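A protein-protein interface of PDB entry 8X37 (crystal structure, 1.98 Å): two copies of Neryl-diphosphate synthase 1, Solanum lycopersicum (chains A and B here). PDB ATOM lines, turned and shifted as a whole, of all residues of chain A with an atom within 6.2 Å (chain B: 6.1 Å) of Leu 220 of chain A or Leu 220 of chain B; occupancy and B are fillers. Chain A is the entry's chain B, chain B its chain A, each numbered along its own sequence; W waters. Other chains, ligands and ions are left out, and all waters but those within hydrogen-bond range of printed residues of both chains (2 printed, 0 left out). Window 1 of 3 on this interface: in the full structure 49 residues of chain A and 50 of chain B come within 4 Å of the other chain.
The backbone NH (N) of Gly 162 of chain B is in hydrogen-bond range of the side-chain amide oxygen (OD1) of Asn 217 of chain B (3.0 Å).
N of Tyr 163 of chain B sits at hydrogen-bond distance from OD1 of Asn 217 of chain B.
The side-chain amide oxygen of Asn 217 of chain A is in hydrogen-bond range of the backbone NH of Gly 162 of chain A, at 3.0 Å.
The side-chain amide oxygen of Asn 217 of chain A lies within hydrogen-bond range of the backbone NH of Tyr 163 of chain A.
O of Ala 224 of chain A is in hydrogen-bond range of N of Ser 216 of chain B, at 3.1 Å.
O of Ala 224 of chain A is in hydrogen-bond range of N of Asn 217 of chain B.
The backbone carbonyl oxygen of Trp 221 of chain B is in hydrogen-bond range of the side-chain hydroxyl of Tyr 163 of chain A (3.0 Å).
The backbone carbonyl oxygen of Ala 224 of chain B is in hydrogen-bond range of the backbone NH of Ser 216 of chain A (3.1 Å).
The backbone carbonyl oxygen of Ala 224 of chain B sits at hydrogen-bond distance from the backbone NH of Asn 217 of chain A (3.0 Å).
Tyr 163 of chain A touches Ala 224 of chain B (OH to CB, 3.1 Å).
Ile 166 of chain B touches Ile 166 of chain A (CD1 to CD1, 3.9 Å).
Trp 221 of chain B touches Ile 166 of chain A (CZ3 to CG2, 3.9 Å).
Val 215 of chain A touches Ala 224 of chain B (CG2 to O, 3.6 Å).
Leu 220 of chain A touches Leu 220 of chain B.
Tyr 163 of chain B touches Trp 221 of chain A.
Trp 221 of chain A touches Ile 166 of chain B (CZ3 to CG2, 3.8 Å).
Trp 221 of chain A touches Leu 220 of chain B (O to CD1, 3.99 Å).
O of Leu 223 of chain A touches CG2 of Val 215 of chain B, at 3.9 Å.
OH of Tyr 163 of chain B touches CB of Ala 224 of chain A, 3.3 Å away.
Water W2 lies within hydrogen-bond range of O of Leu 223 of chain A (2.7 Å), N of Val 215 of chain B (3.0 Å) and O of Ala 224 of chain A (3.1 Å).
Water W1 lies within hydrogen-bond range of the backbone NH (N) of Val 215 of chain A (2.8 Å), the backbone carbonyl oxygen (O) of Leu 223 of chain B (2.8 Å) and the backbone carbonyl oxygen (O) of Ala 224 of chain B (3.2 Å).
Gly 162 of chain A touches none of the printed residues of chain B.
Leu 220 of chain A touches just these residues of chain B: Leu 220 and Ala 224.
Printed residues of chain B within 4 Å of Leu 223 of chain A: Val 215.
Gly 162 of chain B touches none of the printed residues of chain A.
Printed residues of chain A within 4 Å of Ile 166 of chain B: Ile 166 and Trp 221.
Of the printed residues of chain A, Leu 220 of chain B touches Leu 220 (3.8 Å), Trp 221 (3.99 Å) and Ala 224 (3.9 Å).
The nearest printed residue of chain A that does not touch Leu 220 of chain B is Leu 223 of chain A (5.0 Å).
Of the 15 printed residues of chain B, 9 touch a printed residue of chain A.
Hydrophobic or aromatic side chains of chain B that line the printed part of chain A: Tyr 163, Ile 166, Val 215, Leu 220, Trp 221 and Ala 224.
Among the printed residues, 19 pairs touch across the chains.
Tyr 163 of chain A touches Trp 221 of chain B, and with the chains exchanged Trp 221 of chain A touches Tyr 163 of chain B.
Asn 217 of chain A touches Ala 224 of chain B, and with the chains exchanged Ala 224 of chain A touches Asn 217 of chain B.
Leu 220 of chain A touches Ala 224 of chain B, and with the chains exchanged Ala 224 of chain A touches Leu 220 of chain B.
Trp 221 of chain A touches Leu 220 of chain B, but with the chains exchanged Leu 220 of chain A does not touch Trp 221 of chain B (4.1 Å).
Positions printed for both chains: 160, 161, 162, 163, 166, 215, 216, 217, 218, 219, 220, 221, 222, 223 and 224.
Of the 19 pairs that touch across the chains among the printed residues, 18 have their exchanged pair printed and touching as well.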
ATOM      1  N   TYR A 160     -30.365   0.725 -16.639  1.00  0.00           N
ATOM      2  CA  TYR A 160     -28.942   0.986 -16.531  1.00  0.00           C
ATOM      3  C   TYR A 160     -28.693   2.239 -15.705  1.00  0.00           C
ATOM      4  O   TYR A 160     -29.595   3.052 -15.484  1.00  0.00           O
ATOM      5  CB  TYR A 160     -28.355   1.110 -17.938  1.00  0.00           C
ATOM      6  CG  TYR A 160     -26.887   1.503 -17.977  1.00  0.00           C
ATOM      7  CD1 TYR A 160     -26.512   2.837 -17.912  1.00  0.00           C
ATOM      8  CD2 TYR A 160     -25.877   0.552 -18.068  1.00  0.00           C
ATOM      9  CE1 TYR A 160     -25.177   3.210 -17.946  1.00  0.00           C
ATOM     10  CE2 TYR A 160     -24.532   0.914 -18.108  1.00  0.00           C
ATOM     11  CZ  TYR A 160     -24.182   2.248 -18.042  1.00  0.00           C
ATOM     12  OH  TYR A 160     -22.874   2.636 -18.077  1.00  0.00           O
ATOM     13  N   GLY A 161     -27.468   2.303 -15.177  1.00  0.00           N
ATOM     14  CA  GLY A 161     -26.928   3.481 -14.518  1.00  0.00           C
ATOM     15  C   GLY A 161     -25.404   3.400 -14.491  1.00  0.00           C
ATOM     16  O   GLY A 161     -24.836   2.303 -14.527  1.00  0.00           O
ATOM     17  N   GLY A 162     -24.754   4.569 -14.452  1.00  0.00           N
ATOM     18  CA  GLY A 162     -23.311   4.634 -14.330  1.00  0.00           C
ATOM     19  C   GLY A 162     -22.803   4.029 -13.020  1.00  0.00           C
ATOM     20  O   GLY A 162     -21.741   3.403 -12.972  1.00  0.00           O
ATOM     21  N   TYR A 163     -23.550   4.228 -11.937  1.00  0.00           N
ATOM     22  CA  TYR A 163     -23.162   3.653 -10.654  1.00  0.00           C
ATOM     23  C   TYR A 163     -23.164   2.131 -10.767  1.00  0.00           C
ATOM     24  O   TYR A 163     -22.209   1.485 -10.341  1.00  0.00           O
ATOM     25  CB  TYR A 163     -24.079   4.090  -9.498  1.00  0.00           C
ATOM     26  CG  TYR A 163     -23.937   5.546  -9.062  1.00  0.00           C
ATOM     27  CD1 TYR A 163     -22.703   6.186  -9.096  1.00  0.00           C
ATOM     28  CD2 TYR A 163     -25.042   6.302  -8.652  1.00  0.00           C
ATOM     29  CE1 TYR A 163     -22.564   7.513  -8.730  1.00  0.00           C
ATOM     30  CE2 TYR A 163     -24.907   7.623  -8.246  1.00  0.00           C
ATOM     31  CZ  TYR A 163     -23.664   8.233  -8.290  1.00  0.00           C
ATOM     32  OH  TYR A 163     -23.447   9.542  -7.916  1.00  0.00           O
ATOM     33  N   ILE A 166     -20.117   0.712 -12.909  1.00  0.00           N
ATOM     34  CA  ILE A 166     -18.867   0.738 -12.165  1.00  0.00           C
ATOM     35  C   ILE A 166     -18.869  -0.314 -11.050  1.00  0.00           C
ATOM     36  O   ILE A 166     -17.850  -0.978 -10.834  1.00  0.00           O
ATOM     37  CB  ILE A 166     -18.576   2.145 -11.623  1.00  0.00           C
ATOM     38  CG1 ILE A 166     -18.191   3.091 -12.746  1.00  0.00           C
ATOM     39  CG2 ILE A 166     -17.489   2.108 -10.549  1.00  0.00           C
ATOM     40  CD1 ILE A 166     -18.350   4.555 -12.395  1.00  0.00           C
ATOM     41  N   VAL A 215     -26.294  14.832 -16.389  1.00  0.00           N
ATOM     42  CA  VAL A 215     -26.119  13.516 -17.002  1.00  0.00           C
ATOM     43  C   VAL A 215     -27.026  12.466 -16.366  1.00  0.00           C
ATOM     44  O   VAL A 215     -27.153  11.384 -16.921  1.00  0.00           O
ATOM     45  CB  VAL A 215     -24.659  13.017 -17.020  1.00  0.00           C
ATOM     46  CG1 VAL A 215     -23.795  13.879 -17.923  1.00  0.00           C
ATOM     47  CG2 VAL A 215     -24.042  12.909 -15.636  1.00  0.00           C
ATOM     48  N   SER A 216     -27.616  12.752 -15.202  1.00  0.00           N
ATOM     49  CA  SER A 216     -28.579  11.858 -14.581  1.00  0.00           C
ATOM     50  C   SER A 216     -28.117  10.393 -14.590  1.00  0.00           C
ATOM     51  O   SER A 216     -28.877   9.483 -14.945  1.00  0.00           O
ATOM     52  CB  SER A 216     -29.942  12.002 -15.244  1.00  0.00           C
ATOM     53  OG  SER A 216     -30.373  13.356 -15.336  1.00  0.00           O
ATOM     54  N   ASN A 217     -26.879  10.142 -14.137  1.00  0.00           N
ATOM     55  CA  ASN A 217     -26.414   8.792 -13.864  1.00  0.00           C
ATOM     56  C   ASN A 217     -26.432   7.933 -15.134  1.00  0.00           C
ATOM     57  O   ASN A 217     -26.800   6.770 -15.054  1.00  0.00           O
ATOM     58  CB  ASN A 217     -27.236   8.117 -12.761  1.00  0.00           C
ATOM     59  CG  ASN A 217     -26.602   6.848 -12.235  1.00  0.00           C
ATOM     60  OD1 ASN A 217     -25.379   6.656 -12.345  1.00  0.00           O
ATOM     61  ND2 ASN A 217     -27.403   5.996 -11.604  1.00  0.00           N
ATOM     62  N   PHE A 218     -26.030   8.503 -16.278  1.00  0.00           N
ATOM     63  CA  PHE A 218     -25.815   7.747 -17.508  1.00  0.00           C
ATOM     64  C   PHE A 218     -24.381   7.198 -17.492  1.00  0.00           C
ATOM     65  O   PHE A 218     -23.948   6.675 -16.484  1.00  0.00           O
ATOM     66  CB  PHE A 218     -26.166   8.684 -18.673  1.00  0.00           C
ATOM     67  CG  PHE A 218     -26.361   8.042 -20.044  1.00  0.00           C
ATOM     68  CD1 PHE A 218     -26.827   6.739 -20.177  1.00  0.00           C
ATOM     69  CD2 PHE A 218     -26.063   8.749 -21.205  1.00  0.00           C
ATOM     70  CE1 PHE A 218     -27.006   6.168 -21.423  1.00  0.00           C
ATOM     71  CE2 PHE A 218     -26.257   8.172 -22.460  1.00  0.00           C
ATOM     72  CZ  PHE A 218     -26.719   6.881 -22.571  1.00  0.00           C
ATOM     73  N   LEU A 219     -23.607   7.387 -18.567  1.00  0.00           N
ATOM     74  CA  LEU A 219     -22.302   6.765 -18.700  1.00  0.00           C
ATOM     75  C   LEU A 219     -21.221   7.574 -17.973  1.00  0.00           C
ATOM     76  O   LEU A 219     -20.335   8.140 -18.621  1.00  0.00           O
ATOM     77  CB  LEU A 219     -21.946   6.653 -20.189  1.00  0.00           C
ATOM     78  CG  LEU A 219     -22.990   6.032 -21.120  1.00  0.00           C
ATOM     79  CD1 LEU A 219     -22.722   6.391 -22.580  1.00  0.00           C
ATOM     80  CD2 LEU A 219     -23.066   4.545 -20.926  1.00  0.00           C
ATOM     81  N   LEU A 220     -21.189   7.518 -16.640  1.00  0.00           N
ATOM     82  CA  LEU A 220     -20.266   8.306 -15.830  1.00  0.00           C
ATOM     83  C   LEU A 220     -18.784   8.144 -16.211  1.00  0.00           C
ATOM     84  O   LEU A 220     -18.113   9.136 -16.458  1.00  0.00           O
ATOM     85  CB  LEU A 220     -20.506   7.919 -14.378  1.00  0.00           C
ATOM     86  CG  LEU A 220     -21.909   8.225 -13.832  1.00  0.00           C
ATOM     87  CD1 LEU A 220     -21.903   7.981 -12.344  1.00  0.00           C
ATOM     88  CD2 LEU A 220     -22.373   9.652 -14.150  1.00  0.00           C
ATOM     89  N   TRP A 221     -18.241   6.918 -16.229  1.00  0.00           N
ATOM     90  CA  TRP A 221     -16.834   6.686 -16.573  1.00  0.00           C
ATOM     91  C   TRP A 221     -16.547   7.087 -18.023  1.00  0.00           C
ATOM     92  O   TRP A 221     -15.513   7.682 -18.340  1.00  0.00           O
ATOM     93  CB  TRP A 221     -16.511   5.209 -16.310  1.00  0.00           C
ATOM     94  CG  TRP A 221     -15.175   4.714 -16.801  1.00  0.00           C
ATOM     95  CD1 TRP A 221     -14.839   4.405 -18.087  1.00  0.00           C
ATOM     96  CD2 TRP A 221     -14.004   4.446 -16.007  1.00  0.00           C
ATOM     97  NE1 TRP A 221     -13.528   4.017 -18.160  1.00  0.00           N
ATOM     98  CE2 TRP A 221     -12.996   4.017 -16.899  1.00  0.00           C
ATOM     99  CE3 TRP A 221     -13.705   4.538 -14.645  1.00  0.00           C
ATOM    100  CZ2 TRP A 221     -11.719   3.685 -16.471  1.00  0.00           C
ATOM    101  CZ3 TRP A 221     -12.440   4.193 -14.220  1.00  0.00           C
ATOM    102  CH2 TRP A 221     -11.461   3.775 -15.123  1.00  0.00           C
ATOM    103  N   GLN A 222     -17.470   6.735 -18.923  1.00  0.00           N
ATOM    104  CA  GLN A 222     -17.228   6.816 -20.353  1.00  0.00           C
ATOM    105  C   GLN A 222     -17.276   8.256 -20.871  1.00  0.00           C
ATOM    106  O   GLN A 222     -16.747   8.516 -21.944  1.00  0.00           O
ATOM    107  CB  GLN A 222     -18.219   5.904 -21.070  1.00  0.00           C
ATOM    108  CG  GLN A 222     -18.160   4.435 -20.687  1.00  0.00           C
ATOM    109  CD  GLN A 222     -18.931   4.034 -19.444  1.00  0.00           C
ATOM    110  OE1 GLN A 222     -19.517   4.852 -18.723  1.00  0.00           O
ATOM    111  NE2 GLN A 222     -18.936   2.736 -19.169  1.00  0.00           N
ATOM    112  N   LEU A 223     -17.867   9.201 -20.125  1.00  0.00           N
ATOM    113  CA  LEU A 223     -18.074  10.573 -20.599  1.00  0.00           C
ATOM    114  C   LEU A 223     -16.927  11.532 -20.245  1.00  0.00           C
ATOM    115  O   LEU A 223     -17.089  12.754 -20.377  1.00  0.00           O
ATOM    116  CB  LEU A 223     -19.389  11.117 -20.034  1.00  0.00           C
ATOM    117  CG  LEU A 223     -20.664  10.452 -20.558  1.00  0.00           C
ATOM    118  CD1 LEU A 223     -21.866  11.010 -19.817  1.00  0.00           C
ATOM    119  CD2 LEU A 223     -20.850  10.558 -22.085  1.00  0.00           C
ATOM    120  N   ALA A 224     -15.765  10.998 -19.848  1.00  0.00           N
ATOM    121  CA  ALA A 224     -14.707  11.790 -19.248  1.00  0.00           C
ATOM    122  C   ALA A 224     -14.261  12.927 -20.162  1.00  0.00           C
ATOM    123  O   ALA A 224     -13.970  14.016 -19.666  1.00  0.00           O
ATOM    124  CB  ALA A 224     -13.536  10.905 -18.899  1.00  0.00           C
ATOM    125  N   TYR B 160      -5.097  15.215 -10.031  1.00  0.00           N
ATOM    126  CA  TYR B 160      -6.282  14.406  -9.788  1.00  0.00           C
ATOM    127  C   TYR B 160      -6.974  14.094 -11.113  1.00  0.00           C
ATOM    128  O   TYR B 160      -6.730  14.737 -12.138  1.00  0.00           O
ATOM    129  CB  TYR B 160      -7.226  15.127  -8.828  1.00  0.00           C
ATOM    130  CG  TYR B 160      -8.575  14.451  -8.647  1.00  0.00           C
ATOM    131  CD1 TYR B 160      -9.624  14.663  -9.550  1.00  0.00           C
ATOM    132  CD2 TYR B 160      -8.811  13.601  -7.574  1.00  0.00           C
ATOM    133  CE1 TYR B 160     -10.852  14.037  -9.389  1.00  0.00           C
ATOM    134  CE2 TYR B 160     -10.044  12.986  -7.391  1.00  0.00           C
ATOM    135  CZ  TYR B 160     -11.062  13.198  -8.304  1.00  0.00           C
ATOM    136  OH  TYR B 160     -12.255  12.574  -8.133  1.00  0.00           O
ATOM    137  N   GLY B 161      -7.760  13.012 -11.089  1.00  0.00           N
ATOM    138  CA  GLY B 161      -8.610  12.602 -12.197  1.00  0.00           C
ATOM    139  C   GLY B 161      -9.705  11.680 -11.676  1.00  0.00           C
ATOM    140  O   GLY B 161      -9.519  11.009 -10.659  1.00  0.00           O
ATOM    141  N   GLY B 162     -10.854  11.655 -12.360  1.00  0.00           N
ATOM    142  CA  GLY B 162     -11.940  10.762 -11.988  1.00  0.00           C
ATOM    143  C   GLY B 162     -11.557   9.292 -12.186  1.00  0.00           C
ATOM    144  O   GLY B 162     -11.955   8.427 -11.400  1.00  0.00           O
ATOM    145  N   TYR B 163     -10.778   9.016 -13.240  1.00  0.00           N
ATOM    146  CA  TYR B 163     -10.299   7.662 -13.478  1.00  0.00           C
ATOM    147  C   TYR B 163      -9.441   7.206 -12.291  1.00  0.00           C
ATOM    148  O   TYR B 163      -9.644   6.108 -11.762  1.00  0.00           O
ATOM    149  CB  TYR B 163      -9.424   7.552 -14.728  1.00  0.00           C
ATOM    150  CG  TYR B 163     -10.054   7.778 -16.087  1.00  0.00           C
ATOM    151  CD1 TYR B 163     -11.338   7.362 -16.393  1.00  0.00           C
ATOM    152  CD2 TYR B 163      -9.315   8.395 -17.087  1.00  0.00           C
ATOM    153  CE1 TYR B 163     -11.871   7.535 -17.667  1.00  0.00           C
ATOM    154  CE2 TYR B 163      -9.847   8.624 -18.339  1.00  0.00           C
ATOM    155  CZ  TYR B 163     -11.121   8.178 -18.641  1.00  0.00           C
ATOM    156  OH  TYR B 163     -11.586   8.422 -19.903  1.00  0.00           O
ATOM    157  N   ILE B 166     -11.558   6.530  -8.999  1.00  0.00           N
ATOM    158  CA  ILE B 166     -12.307   5.280  -9.070  1.00  0.00           C
ATOM    159  C   ILE B 166     -11.359   4.080  -8.983  1.00  0.00           C
ATOM    160  O   ILE B 166     -11.692   3.112  -8.305  1.00  0.00           O
ATOM    161  CB  ILE B 166     -13.179   5.238 -10.342  1.00  0.00           C
ATOM    162  CG1 ILE B 166     -14.384   6.176 -10.191  1.00  0.00           C
ATOM    163  CG2 ILE B 166     -13.633   3.819 -10.666  1.00  0.00           C
ATOM    164  CD1 ILE B 166     -15.070   6.536 -11.487  1.00  0.00           C
ATOM    165  N   VAL B 215     -16.385  17.705 -19.080  1.00  0.00           N
ATOM    166  CA  VAL B 215     -15.977  17.612 -17.681  1.00  0.00           C
ATOM    167  C   VAL B 215     -14.486  17.288 -17.551  1.00  0.00           C
ATOM    168  O   VAL B 215     -13.946  17.357 -16.460  1.00  0.00           O
ATOM    169  CB  VAL B 215     -16.816  16.631 -16.847  1.00  0.00           C
ATOM    170  CG1 VAL B 215     -18.255  17.099 -16.744  1.00  0.00           C
ATOM    171  CG2 VAL B 215     -16.762  15.182 -17.337  1.00  0.00           C
ATOM    172  N   SER B 216     -13.822  16.946 -18.645  1.00  0.00           N
ATOM    173  CA  SER B 216     -12.376  16.767 -18.676  1.00  0.00           C
ATOM    174  C   SER B 216     -11.851  15.916 -17.508  1.00  0.00           C
ATOM    175  O   SER B 216     -10.858  16.252 -16.883  1.00  0.00           O
ATOM    176  CB  SER B 216     -11.712  18.125 -18.774  1.00  0.00           C
ATOM    177  OG  SER B 216     -11.957  18.761 -20.034  1.00  0.00           O
ATOM    178  N   ASN B 217     -12.491  14.775 -17.226  1.00  0.00           N
ATOM    179  CA  ASN B 217     -11.983  13.799 -16.257  1.00  0.00           C
ATOM    180  C   ASN B 217     -11.864  14.396 -14.852  1.00  0.00           C
ATOM    181  O   ASN B 217     -10.919  14.091 -14.133  1.00  0.00           O
ATOM    182  CB  ASN B 217     -10.648  13.200 -16.697  1.00  0.00           C
ATOM    183  CG  ASN B 217     -10.247  11.962 -15.919  1.00  0.00           C
ATOM    184  OD1 ASN B 217     -11.077  11.273 -15.311  1.00  0.00           O
ATOM    185  ND2 ASN B 217      -8.967  11.637 -15.938  1.00  0.00           N
ATOM    186  N   PHE B 218     -12.843  15.215 -14.445  1.00  0.00           N
ATOM    187  CA  PHE B 218     -12.953  15.707 -13.081  1.00  0.00           C
ATOM    188  C   PHE B 218     -13.679  14.662 -12.238  1.00  0.00           C
ATOM    189  O   PHE B 218     -13.369  13.484 -12.352  1.00  0.00           O
ATOM    190  CB  PHE B 218     -13.588  17.107 -13.162  1.00  0.00           C
ATOM    191  CG  PHE B 218     -13.467  17.989 -11.928  1.00  0.00           C
ATOM    192  CD1 PHE B 218     -12.363  17.881 -11.075  1.00  0.00           C
ATOM    193  CD2 PHE B 218     -14.468  18.897 -11.586  1.00  0.00           C
ATOM    194  CE1 PHE B 218     -12.255  18.665  -9.938  1.00  0.00           C
ATOM    195  CE2 PHE B 218     -14.346  19.702 -10.454  1.00  0.00           C
ATOM    196  CZ  PHE B 218     -13.251  19.569  -9.621  1.00  0.00           C
ATOM    197  N   LEU B 219     -14.655  15.072 -11.413  1.00  0.00           N
ATOM    198  CA  LEU B 219     -15.300  14.178 -10.462  1.00  0.00           C
ATOM    199  C   LEU B 219     -16.373  13.315 -11.133  1.00  0.00           C
ATOM    200  O   LEU B 219     -17.560  13.495 -10.851  1.00  0.00           O
ATOM    201  CB  LEU B 219     -15.938  15.014  -9.342  1.00  0.00           C
ATOM    202  CG  LEU B 219     -15.074  16.078  -8.665  1.00  0.00           C
ATOM    203  CD1 LEU B 219     -15.943  17.118  -7.934  1.00  0.00           C
ATOM    204  CD2 LEU B 219     -14.111  15.418  -7.710  1.00  0.00           C
ATOM    205  N   LEU B 220     -15.968  12.284 -11.898  1.00  0.00           N
ATOM    206  CA  LEU B 220     -16.898  11.499 -12.712  1.00  0.00           C
ATOM    207  C   LEU B 220     -18.019  10.844 -11.890  1.00  0.00           C
ATOM    208  O   LEU B 220     -19.186  10.974 -12.234  1.00  0.00           O
ATOM    209  CB  LEU B 220     -16.110  10.465 -13.493  1.00  0.00           C
ATOM    210  CG  LEU B 220     -15.034  11.008 -14.445  1.00  0.00           C
ATOM    211  CD1 LEU B 220     -14.364   9.885 -15.222  1.00  0.00           C
ATOM    212  CD2 LEU B 220     -15.624  11.983 -15.407  1.00  0.00           C
ATOM    213  N   TRP B 221     -17.693  10.111 -10.822  1.00  0.00           N
ATOM    214  CA  TRP B 221     -18.705   9.456 -10.000  1.00  0.00           C
ATOM    215  C   TRP B 221     -19.595  10.480  -9.293  1.00  0.00           C
ATOM    216  O   TRP B 221     -20.812  10.312  -9.188  1.00  0.00           O
ATOM    217  CB  TRP B 221     -17.994   8.523  -9.003  1.00  0.00           C
ATOM    218  CG  TRP B 221     -18.843   7.896  -7.927  1.00  0.00           C
ATOM    219  CD1 TRP B 221     -19.295   8.516  -6.807  1.00  0.00           C
ATOM    220  CD2 TRP B 221     -19.295   6.529  -7.833  1.00  0.00           C
ATOM    221  NE1 TRP B 221     -20.040   7.653  -6.046  1.00  0.00           N
ATOM    222  CE2 TRP B 221     -20.045   6.424  -6.637  1.00  0.00           C
ATOM    223  CE3 TRP B 221     -19.168   5.396  -8.640  1.00  0.00           C
ATOM    224  CZ2 TRP B 221     -20.641   5.242  -6.228  1.00  0.00           C
ATOM    225  CZ3 TRP B 221     -19.783   4.232  -8.244  1.00  0.00           C
ATOM    226  CH2 TRP B 221     -20.505   4.150  -7.053  1.00  0.00           C
ATOM    227  N   GLN B 222     -18.965  11.523  -8.752  1.00  0.00           N
ATOM    228  CA  GLN B 222     -19.626  12.449  -7.856  1.00  0.00           C
ATOM    229  C   GLN B 222     -20.576  13.405  -8.602  1.00  0.00           C
ATOM    230  O   GLN B 222     -21.487  13.946  -7.986  1.00  0.00           O
ATOM    231  CB  GLN B 222     -18.559  13.198  -7.055  1.00  0.00           C
ATOM    232  CG  GLN B 222     -17.652  12.301  -6.226  1.00  0.00           C
ATOM    233  CD  GLN B 222     -16.418  11.802  -6.951  1.00  0.00           C
ATOM    234  OE1 GLN B 222     -16.254  11.939  -8.174  1.00  0.00           O
ATOM    235  NE2 GLN B 222     -15.520  11.209  -6.167  1.00  0.00           N
ATOM    236  N   LEU B 223     -20.409  13.583  -9.921  1.00  0.00           N
ATOM    237  CA  LEU B 223     -21.244  14.482 -10.709  1.00  0.00           C
ATOM    238  C   LEU B 223     -22.508  13.835 -11.295  1.00  0.00           C
ATOM    239  O   LEU B 223     -23.132  14.429 -12.175  1.00  0.00           O
ATOM    240  CB  LEU B 223     -20.389  15.057 -11.838  1.00  0.00           C
ATOM    241  CG  LEU B 223     -19.278  16.012 -11.416  1.00  0.00           C
ATOM    242  CD1 LEU B 223     -18.429  16.382 -12.620  1.00  0.00           C
ATOM    243  CD2 LEU B 223     -19.834  17.270 -10.738  1.00  0.00           C
ATOM    244  N   ALA B 224     -22.918  12.659 -10.798  1.00  0.00           N
ATOM    245  CA  ALA B 224     -23.951  11.874 -11.447  1.00  0.00           C
ATOM    246  C   ALA B 224     -25.265  12.647 -11.581  1.00  0.00           C
ATOM    247  O   ALA B 224     -25.943  12.484 -12.595  1.00  0.00           O
ATOM    248  CB  ALA B 224     -24.186  10.603 -10.684  1.00  0.00           C
HETATM  249  O   HOH W   1     -25.257  15.358 -13.811  1.00  0.00           O
HETATM  250  O   HOH W   2     -16.500  15.364 -20.875  1.00  0.00           O
